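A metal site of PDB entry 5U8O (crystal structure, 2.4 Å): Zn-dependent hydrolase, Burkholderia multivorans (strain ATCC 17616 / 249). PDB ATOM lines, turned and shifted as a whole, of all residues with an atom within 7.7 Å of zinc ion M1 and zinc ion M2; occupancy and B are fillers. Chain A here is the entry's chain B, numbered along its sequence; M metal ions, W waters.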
ATOM      1  N   HIS A   7     -29.482  -6.784 -32.253  1.00  0.00           N
ATOM      2  CA  HIS A   7     -30.460  -6.085 -31.438  1.00  0.00           C
ATOM      3  C   HIS A   7     -31.871  -6.565 -31.761  1.00  0.00           C
ATOM      4  O   HIS A   7     -32.149  -7.053 -32.866  1.00  0.00           O
ATOM      5  CB  HIS A   7     -30.358  -4.573 -31.631  1.00  0.00           C
ATOM      6  CG  HIS A   7     -28.974  -4.024 -31.444  1.00  0.00           C
ATOM      7  ND1 HIS A   7     -28.027  -4.029 -32.455  1.00  0.00           N
ATOM      8  CD2 HIS A   7     -28.374  -3.483 -30.359  1.00  0.00           C
ATOM      9  CE1 HIS A   7     -26.900  -3.503 -31.997  1.00  0.00           C
ATOM     10  NE2 HIS A   7     -27.084  -3.163 -30.723  1.00  0.00           N
ATOM     11  N   LEU A  44     -21.427   6.029 -35.933  1.00  0.00           N
ATOM     12  CA  LEU A  44     -20.657   4.863 -35.503  1.00  0.00           C
ATOM     13  C   LEU A  44     -20.611   3.879 -36.655  1.00  0.00           C
ATOM     14  O   LEU A  44     -21.561   3.766 -37.434  1.00  0.00           O
ATOM     15  CB  LEU A  44     -21.272   4.175 -34.276  1.00  0.00           C
ATOM     16  CG  LEU A  44     -21.280   4.982 -32.983  1.00  0.00           C
ATOM     17  CD1 LEU A  44     -21.889   4.139 -31.875  1.00  0.00           C
ATOM     18  CD2 LEU A  44     -19.872   5.407 -32.630  1.00  0.00           C
ATOM     19  N   LEU A  48     -25.359  -0.609 -35.242  1.00  0.00           N
ATOM     20  CA  LEU A  48     -25.869   0.547 -34.517  1.00  0.00           C
ATOM     21  C   LEU A  48     -25.061   1.761 -34.981  1.00  0.00           C
ATOM     22  O   LEU A  48     -23.906   1.956 -34.594  1.00  0.00           O
ATOM     23  CB  LEU A  48     -25.734   0.275 -33.015  1.00  0.00           C
ATOM     24  CG  LEU A  48     -26.549   1.126 -32.048  1.00  0.00           C
ATOM     25  CD1 LEU A  48     -27.968   1.374 -32.583  1.00  0.00           C
ATOM     26  CD2 LEU A  48     -26.585   0.379 -30.714  1.00  0.00           C
ATOM     27  N   HIS A  50     -24.958   5.013 -34.692  1.00  0.00           N
ATOM     28  CA  HIS A  50     -24.923   6.336 -34.092  1.00  0.00           C
ATOM     29  C   HIS A  50     -24.949   6.214 -32.570  1.00  0.00           C
ATOM     30  O   HIS A  50     -25.385   5.202 -32.019  1.00  0.00           O
ATOM     31  CB  HIS A  50     -26.126   7.171 -34.534  1.00  0.00           C
ATOM     32  CG  HIS A  50     -27.416   6.703 -33.925  1.00  0.00           C
ATOM     33  ND1 HIS A  50     -28.138   5.646 -34.437  1.00  0.00           N
ATOM     34  CD2 HIS A  50     -28.053   7.081 -32.783  1.00  0.00           C
ATOM     35  CE1 HIS A  50     -29.191   5.431 -33.673  1.00  0.00           C
ATOM     36  NE2 HIS A  50     -29.164   6.280 -32.660  1.00  0.00           N
ATOM     37  N   ILE A  51     -24.509   7.280 -31.903  1.00  0.00           N
ATOM     38  CA  ILE A  51     -24.736   7.476 -30.481  1.00  0.00           C
ATOM     39  C   ILE A  51     -25.120   8.928 -30.295  1.00  0.00           C
ATOM     40  O   ILE A  51     -24.590   9.823 -30.968  1.00  0.00           O
ATOM     41  CB  ILE A  51     -23.487   7.110 -29.630  1.00  0.00           C
ATOM     42  CG1 ILE A  51     -23.807   7.256 -28.135  1.00  0.00           C
ATOM     43  CG2 ILE A  51     -22.249   7.973 -30.024  1.00  0.00           C
ATOM     44  CD1 ILE A  51     -22.705   6.670 -27.160  1.00  0.00           C
ATOM     45  N   ASP A  70     -21.155  11.914 -22.242  1.00  0.00           N
ATOM     46  CA  ASP A  70     -20.666  10.872 -23.165  1.00  0.00           C
ATOM     47  C   ASP A  70     -19.898  11.441 -24.370  1.00  0.00           C
ATOM     48  O   ASP A  70     -19.998  12.647 -24.666  1.00  0.00           O
ATOM     49  CB  ASP A  70     -21.814   9.958 -23.598  1.00  0.00           C
ATOM     50  CG  ASP A  70     -22.227   8.975 -22.493  1.00  0.00           C
ATOM     51  OD1 ASP A  70     -21.534   8.924 -21.457  1.00  0.00           O
ATOM     52  OD2 ASP A  70     -23.229   8.247 -22.673  1.00  0.00           O
ATOM     53  N   THR A 101     -21.587   7.885 -18.775  1.00  0.00           N
ATOM     54  CA  THR A 101     -22.589   7.011 -18.182  1.00  0.00           C
ATOM     55  C   THR A 101     -22.042   5.610 -17.908  1.00  0.00           C
ATOM     56  O   THR A 101     -22.379   5.015 -16.884  1.00  0.00           O
ATOM     57  CB  THR A 101     -23.805   6.936 -19.115  1.00  0.00           C
ATOM     58  OG1 THR A 101     -23.388   6.437 -20.398  1.00  0.00           O
ATOM     59  CG2 THR A 101     -24.470   8.310 -19.279  1.00  0.00           C
ATOM     60  N   HIS A 102     -21.221   5.067 -18.796  1.00  0.00           N
ATOM     61  CA  HIS A 102     -20.632   3.741 -18.591  1.00  0.00           C
ATOM     62  C   HIS A 102     -19.412   3.545 -19.499  1.00  0.00           C
ATOM     63  O   HIS A 102     -19.110   4.373 -20.375  1.00  0.00           O
ATOM     64  CB  HIS A 102     -21.666   2.621 -18.779  1.00  0.00           C
ATOM     65  CG  HIS A 102     -22.299   2.545 -20.139  1.00  0.00           C
ATOM     66  ND1 HIS A 102     -22.932   3.607 -20.738  1.00  0.00           N
ATOM     67  CD2 HIS A 102     -22.451   1.500 -20.989  1.00  0.00           C
ATOM     68  CE1 HIS A 102     -23.433   3.233 -21.896  1.00  0.00           C
ATOM     69  NE2 HIS A 102     -23.144   1.957 -22.086  1.00  0.00           N
ATOM     70  N   CYS A 103     -18.704   2.435 -19.261  1.00  0.00           N
ATOM     71  CA  CYS A 103     -17.383   2.247 -19.843  1.00  0.00           C
ATOM     72  C   CYS A 103     -17.404   1.862 -21.317  1.00  0.00           C
ATOM     73  O   CYS A 103     -16.334   1.736 -21.926  1.00  0.00           O
ATOM     74  CB  CYS A 103     -16.617   1.198 -19.059  1.00  0.00           C
ATOM     75  SG  CYS A 103     -17.262  -0.440 -19.345  1.00  0.00           S
ATOM     76  N   HIS A 104     -18.561   1.654 -21.923  1.00  0.00           N
ATOM     77  CA  HIS A 104     -18.555   1.066 -23.250  1.00  0.00           C
ATOM     78  C   HIS A 104     -17.945   2.015 -24.287  1.00  0.00           C
ATOM     79  O   HIS A 104     -18.006   3.242 -24.131  1.00  0.00           O
ATOM     80  CB  HIS A 104     -19.952   0.619 -23.637  1.00  0.00           C
ATOM     81  CG  HIS A 104     -20.398  -0.575 -22.830  1.00  0.00           C
ATOM     82  ND1 HIS A 104     -21.670  -1.100 -22.892  1.00  0.00           N
ATOM     83  CD2 HIS A 104     -19.715  -1.310 -21.923  1.00  0.00           C
ATOM     84  CE1 HIS A 104     -21.746  -2.134 -22.069  1.00  0.00           C
ATOM     85  NE2 HIS A 104     -20.573  -2.280 -21.460  1.00  0.00           N
ATOM     86  N   PRO A 105     -17.299   1.461 -25.309  1.00  0.00           N
ATOM     87  CA  PRO A 105     -16.388   2.286 -26.118  1.00  0.00           C
ATOM     88  C   PRO A 105     -17.033   3.488 -26.766  1.00  0.00           C
ATOM     89  O   PRO A 105     -16.369   4.537 -26.884  1.00  0.00           O
ATOM     90  CB  PRO A 105     -15.871   1.294 -27.171  1.00  0.00           C
ATOM     91  CG  PRO A 105     -16.113  -0.061 -26.602  1.00  0.00           C
ATOM     92  CD  PRO A 105     -17.323   0.055 -25.734  1.00  0.00           C
ATOM     93  N   ASP A 106     -18.304   3.398 -27.157  1.00  0.00           N
ATOM     94  CA  ASP A 106     -18.971   4.530 -27.804  1.00  0.00           C
ATOM     95  C   ASP A 106     -19.347   5.641 -26.834  1.00  0.00           C
ATOM     96  O   ASP A 106     -19.642   6.752 -27.281  1.00  0.00           O
ATOM     97  CB  ASP A 106     -20.228   4.086 -28.578  1.00  0.00           C
ATOM     98  CG  ASP A 106     -21.097   3.060 -27.812  1.00  0.00           C
ATOM     99  OD1 ASP A 106     -22.339   3.205 -27.856  1.00  0.00           O
ATOM    100  OD2 ASP A 106     -20.549   2.153 -27.146  1.00  0.00           O
ATOM    101  N   HIS A 107     -19.372   5.367 -25.527  1.00  0.00           N
ATOM    102  CA  HIS A 107     -19.622   6.400 -24.523  1.00  0.00           C
ATOM    103  C   HIS A 107     -18.339   6.966 -23.921  1.00  0.00           C
ATOM    104  O   HIS A 107     -18.326   8.123 -23.478  1.00  0.00           O
ATOM    105  CB  HIS A 107     -20.504   5.833 -23.406  1.00  0.00           C
ATOM    106  CG  HIS A 107     -21.791   5.249 -23.894  1.00  0.00           C
ATOM    107  ND1 HIS A 107     -23.006   5.887 -23.728  1.00  0.00           N
ATOM    108  CD2 HIS A 107     -22.066   4.100 -24.564  1.00  0.00           C
ATOM    109  CE1 HIS A 107     -23.965   5.150 -24.272  1.00  0.00           C
ATOM    110  NE2 HIS A 107     -23.420   4.062 -24.788  1.00  0.00           N
ATOM    111  N   HIS A 213     -26.365  -4.167 -17.467  1.00  0.00           N
ATOM    112  CA  HIS A 213     -25.820  -3.809 -18.762  1.00  0.00           C
ATOM    113  C   HIS A 213     -24.321  -3.543 -18.668  1.00  0.00           C
ATOM    114  O   HIS A 213     -23.568  -3.822 -19.607  1.00  0.00           O
ATOM    115  CB  HIS A 213     -26.530  -2.591 -19.315  1.00  0.00           C
ATOM    116  CG  HIS A 213     -25.923  -2.085 -20.575  1.00  0.00           C
ATOM    117  ND1 HIS A 213     -25.991  -2.778 -21.757  1.00  0.00           N
ATOM    118  CD2 HIS A 213     -25.169  -0.991 -20.820  1.00  0.00           C
ATOM    119  CE1 HIS A 213     -25.345  -2.111 -22.687  1.00  0.00           C
ATOM    120  NE2 HIS A 213     -24.844  -1.017 -22.143  1.00  0.00           N
ATOM    121  N   SER A 214     -23.896  -2.986 -17.546  1.00  0.00           N
ATOM    122  CA  SER A 214     -22.520  -2.595 -17.326  1.00  0.00           C
ATOM    123  C   SER A 214     -22.303  -2.519 -15.825  1.00  0.00           C
ATOM    124  O   SER A 214     -23.268  -2.592 -15.060  1.00  0.00           O
ATOM    125  CB  SER A 214     -22.217  -1.253 -18.020  1.00  0.00           C
ATOM    126  OG  SER A 214     -23.062  -0.254 -17.490  1.00  0.00           O
ATOM    127  N   HIS A 217     -23.939   1.563 -14.191  1.00  0.00           N
ATOM    128  CA  HIS A 217     -24.359   2.535 -15.209  1.00  0.00           C
ATOM    129  C   HIS A 217     -24.971   3.773 -14.558  1.00  0.00           C
ATOM    130  O   HIS A 217     -25.816   3.664 -13.668  1.00  0.00           O
ATOM    131  CB  HIS A 217     -25.361   1.859 -16.148  1.00  0.00           C
ATOM    132  CG  HIS A 217     -25.872   2.737 -17.237  1.00  0.00           C
ATOM    133  ND1 HIS A 217     -26.796   3.739 -17.010  1.00  0.00           N
ATOM    134  CD2 HIS A 217     -25.690   2.687 -18.587  1.00  0.00           C
ATOM    135  CE1 HIS A 217     -27.106   4.315 -18.166  1.00  0.00           C
ATOM    136  NE2 HIS A 217     -26.452   3.691 -19.130  1.00  0.00           N
ATOM    137  N   GLY A 231     -28.985   6.894 -20.766  1.00  0.00           N
ATOM    138  CA  GLY A 231     -27.830   6.137 -21.234  1.00  0.00           C
ATOM    139  C   GLY A 231     -28.280   4.976 -22.105  1.00  0.00           C
ATOM    140  O   GLY A 231     -29.102   5.140 -23.011  1.00  0.00           O
ATOM    141  N   ASP A 232     -27.785   3.779 -21.796  1.00  0.00           N
ATOM    142  CA  ASP A 232     -28.200   2.585 -22.505  1.00  0.00           C
ATOM    143  C   ASP A 232     -29.296   1.799 -21.812  1.00  0.00           C
ATOM    144  O   ASP A 232     -29.730   0.788 -22.374  1.00  0.00           O
ATOM    145  CB  ASP A 232     -26.999   1.670 -22.707  1.00  0.00           C
ATOM    146  CG  ASP A 232     -26.261   1.945 -24.014  1.00  0.00           C
ATOM    147  OD1 ASP A 232     -26.682   2.834 -24.786  1.00  0.00           O
ATOM    148  OD2 ASP A 232     -25.245   1.282 -24.257  1.00  0.00           O
ATOM    149  N   MET A 233     -29.780   2.246 -20.636  1.00  0.00           N
ATOM    150  CA  MET A 233     -30.694   1.399 -19.856  1.00  0.00           C
ATOM    151  C   MET A 233     -32.094   1.347 -20.418  1.00  0.00           C
ATOM    152  O   MET A 233     -32.758   0.309 -20.320  1.00  0.00           O
ATOM    153  CB  MET A 233     -30.756   1.862 -18.401  1.00  0.00           C
ATOM    154  CG  MET A 233     -29.477   1.579 -17.605  1.00  0.00           C
ATOM    155  SD  MET A 233     -29.103  -0.181 -17.395  1.00  0.00           S
ATOM    156  CE  MET A 233     -30.405  -0.712 -16.255  1.00  0.00           C
ATOM    157  N   LEU A 235     -33.855   2.316 -24.068  1.00  0.00           N
ATOM    158  CA  LEU A 235     -33.762   2.701 -25.475  1.00  0.00           C
ATOM    159  C   LEU A 235     -35.085   2.414 -26.170  1.00  0.00           C
ATOM    160  O   LEU A 235     -35.656   1.329 -25.984  1.00  0.00           O
ATOM    161  CB  LEU A 235     -32.626   1.932 -26.187  1.00  0.00           C
ATOM    162  CG  LEU A 235     -31.265   1.997 -25.458  1.00  0.00           C
ATOM    163  CD1 LEU A 235     -30.214   1.022 -26.002  1.00  0.00           C
ATOM    164  CD2 LEU A 235     -30.724   3.437 -25.458  1.00  0.00           C
ATOM    165  N   ILE A 238     -34.500  -0.465 -29.444  1.00  0.00           N
ATOM    166  CA  ILE A 238     -33.776  -1.714 -29.275  1.00  0.00           C
ATOM    167  C   ILE A 238     -33.754  -2.066 -27.800  1.00  0.00           C
ATOM    168  O   ILE A 238     -33.967  -1.243 -26.915  1.00  0.00           O
ATOM    169  CB  ILE A 238     -32.337  -1.637 -29.826  1.00  0.00           C
ATOM    170  CG1 ILE A 238     -31.592  -0.450 -29.204  1.00  0.00           C
ATOM    171  CG2 ILE A 238     -32.361  -1.472 -31.341  1.00  0.00           C
ATOM    172  CD1 ILE A 238     -30.161  -0.337 -29.688  1.00  0.00           C
ATOM    173  N   THR A 240     -31.684  -3.440 -24.444  1.00  0.00           N
ATOM    174  CA  THR A 240     -30.383  -3.202 -23.854  1.00  0.00           C
ATOM    175  C   THR A 240     -29.645  -4.529 -23.776  1.00  0.00           C
ATOM    176  O   THR A 240     -30.204  -5.514 -23.295  1.00  0.00           O
ATOM    177  CB  THR A 240     -30.564  -2.610 -22.472  1.00  0.00           C
ATOM    178  OG1 THR A 240     -31.332  -1.418 -22.597  1.00  0.00           O
ATOM    179  CG2 THR A 240     -29.217  -2.323 -21.853  1.00  0.00           C
ATOM    180  N   ASN A 241     -28.408  -4.556 -24.267  1.00  0.00           N
ATOM    181  CA  ASN A 241     -27.615  -5.788 -24.221  1.00  0.00           C
ATOM    182  C   ASN A 241     -27.317  -6.195 -22.773  1.00  0.00           C
ATOM    183  O   ASN A 241     -26.914  -5.371 -21.953  1.00  0.00           O
ATOM    184  CB  ASN A 241     -26.302  -5.607 -24.994  1.00  0.00           C
ATOM    185  CG  ASN A 241     -25.352  -6.802 -24.841  1.00  0.00           C
ATOM    186  OD1 ASN A 241     -25.480  -7.801 -25.555  1.00  0.00           O
ATOM    187  ND2 ASN A 241     -24.410  -6.698 -23.918  1.00  0.00           N
ATOM    188  N   SER A 276     -29.428   6.975 -25.405  1.00  0.00           N
ATOM    189  CA  SER A 276     -28.185   7.027 -26.150  1.00  0.00           C
ATOM    190  C   SER A 276     -28.315   6.565 -27.597  1.00  0.00           C
ATOM    191  O   SER A 276     -27.414   6.845 -28.404  1.00  0.00           O
ATOM    192  CB  SER A 276     -27.114   6.216 -25.423  1.00  0.00           C
ATOM    193  OG  SER A 276     -26.794   6.911 -24.251  1.00  0.00           O
ATOM    194  N   HIS A 277     -29.380   5.829 -27.932  1.00  0.00           N
ATOM    195  CA  HIS A 277     -29.676   5.422 -29.295  1.00  0.00           C
ATOM    196  C   HIS A 277     -31.173   5.541 -29.529  1.00  0.00           C
ATOM    197  O   HIS A 277     -31.969   5.197 -28.644  1.00  0.00           O
ATOM    198  CB  HIS A 277     -29.198   3.989 -29.577  1.00  0.00           C
ATOM    199  CG  HIS A 277     -27.823   3.726 -29.061  1.00  0.00           C
ATOM    200  ND1 HIS A 277     -26.681   4.060 -29.755  1.00  0.00           N
ATOM    201  CD2 HIS A 277     -27.406   3.218 -27.875  1.00  0.00           C
ATOM    202  CE1 HIS A 277     -25.625   3.739 -29.042  1.00  0.00           C
ATOM    203  NE2 HIS A 277     -26.039   3.230 -27.893  1.00  0.00           N
HETATM  204 ZN    ZN M   1     -24.350   2.313 -26.174  1.00  0.00          ZN
HETATM  205 ZN    ZN M   2     -23.559   0.185 -23.548  1.00  0.00          ZN
HETATM  206  O   HOH W   1     -22.156   0.165 -25.935  1.00  0.00           O
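N of Asp 232 is in hydrogen-bond range of NE2 of His 217, at 3.0 Å. The backbone carbonyl oxygen of Asp 232 is in hydrogen-bond range of the side-chain hydroxyl of Thr 240 (2.7 Å). ND1 of His 213 lies within hydrogen-bond range of O of Asn 241 (2.8 Å). OG1 of Thr 101 is in hydrogen-bond range of ND1 of His 102. The side-chain carboxylate (OD1) of Asp 106 lies close to a ring nitrogen (NE2) of His 107 (3.4 Å). The side-chain carboxylate (OD2) of Asp 70 lies within hydrogen-bond range of a ring nitrogen (ND1) of His 107 (2.6 Å). OG1 of Thr 101 sits at hydrogen-bond distance from ND1 of His 107, at 3.4 Å. The backbone carbonyl oxygen of His 50 is in hydrogen-bond range of a ring nitrogen (ND1) of His 277 (2.8 Å).
Within 4 Å of zinc ion M1: Asp 106, His 107, Asp 232 and His 277. The nearest printed residue that does not touch zinc ion M1 is His 102 (4.3 Å).
Of the 25 residues printed, 4 come within 4 Å of zinc ion M2. The nearest printed residue that does not touch zinc ion M2 is His 107 (4.1 Å).
Zinc ion M1 is bound by the side-chain carboxylate of Asp 232 (2.4 Å), a ring nitrogen (NE2) of His 107 (2.4 Å) and a ring nitrogen (NE2) of His 277 (2.6 Å). Slightly farther from zinc ion M1 lies the side-chain carboxylate (OD1) of Asp 232 (2.8 Å). Slightly farther from zinc ion M1 lies OD1 of Asp 106 (2.8 Å).
Zinc ion M2 is bound by the side-chain carboxylate of Asp 232 (2.1 Å), a ring nitrogen (NE2) of His 213 (2.3 Å), a ring nitrogen (NE2) of His 102 (2.3 Å) and a ring nitrogen (ND1) of His 104 (2.4 Å). Zinc ion M2 has four donor atoms within binding distance. Slightly farther from zinc ion M2 lies water W1 (2.8 Å).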
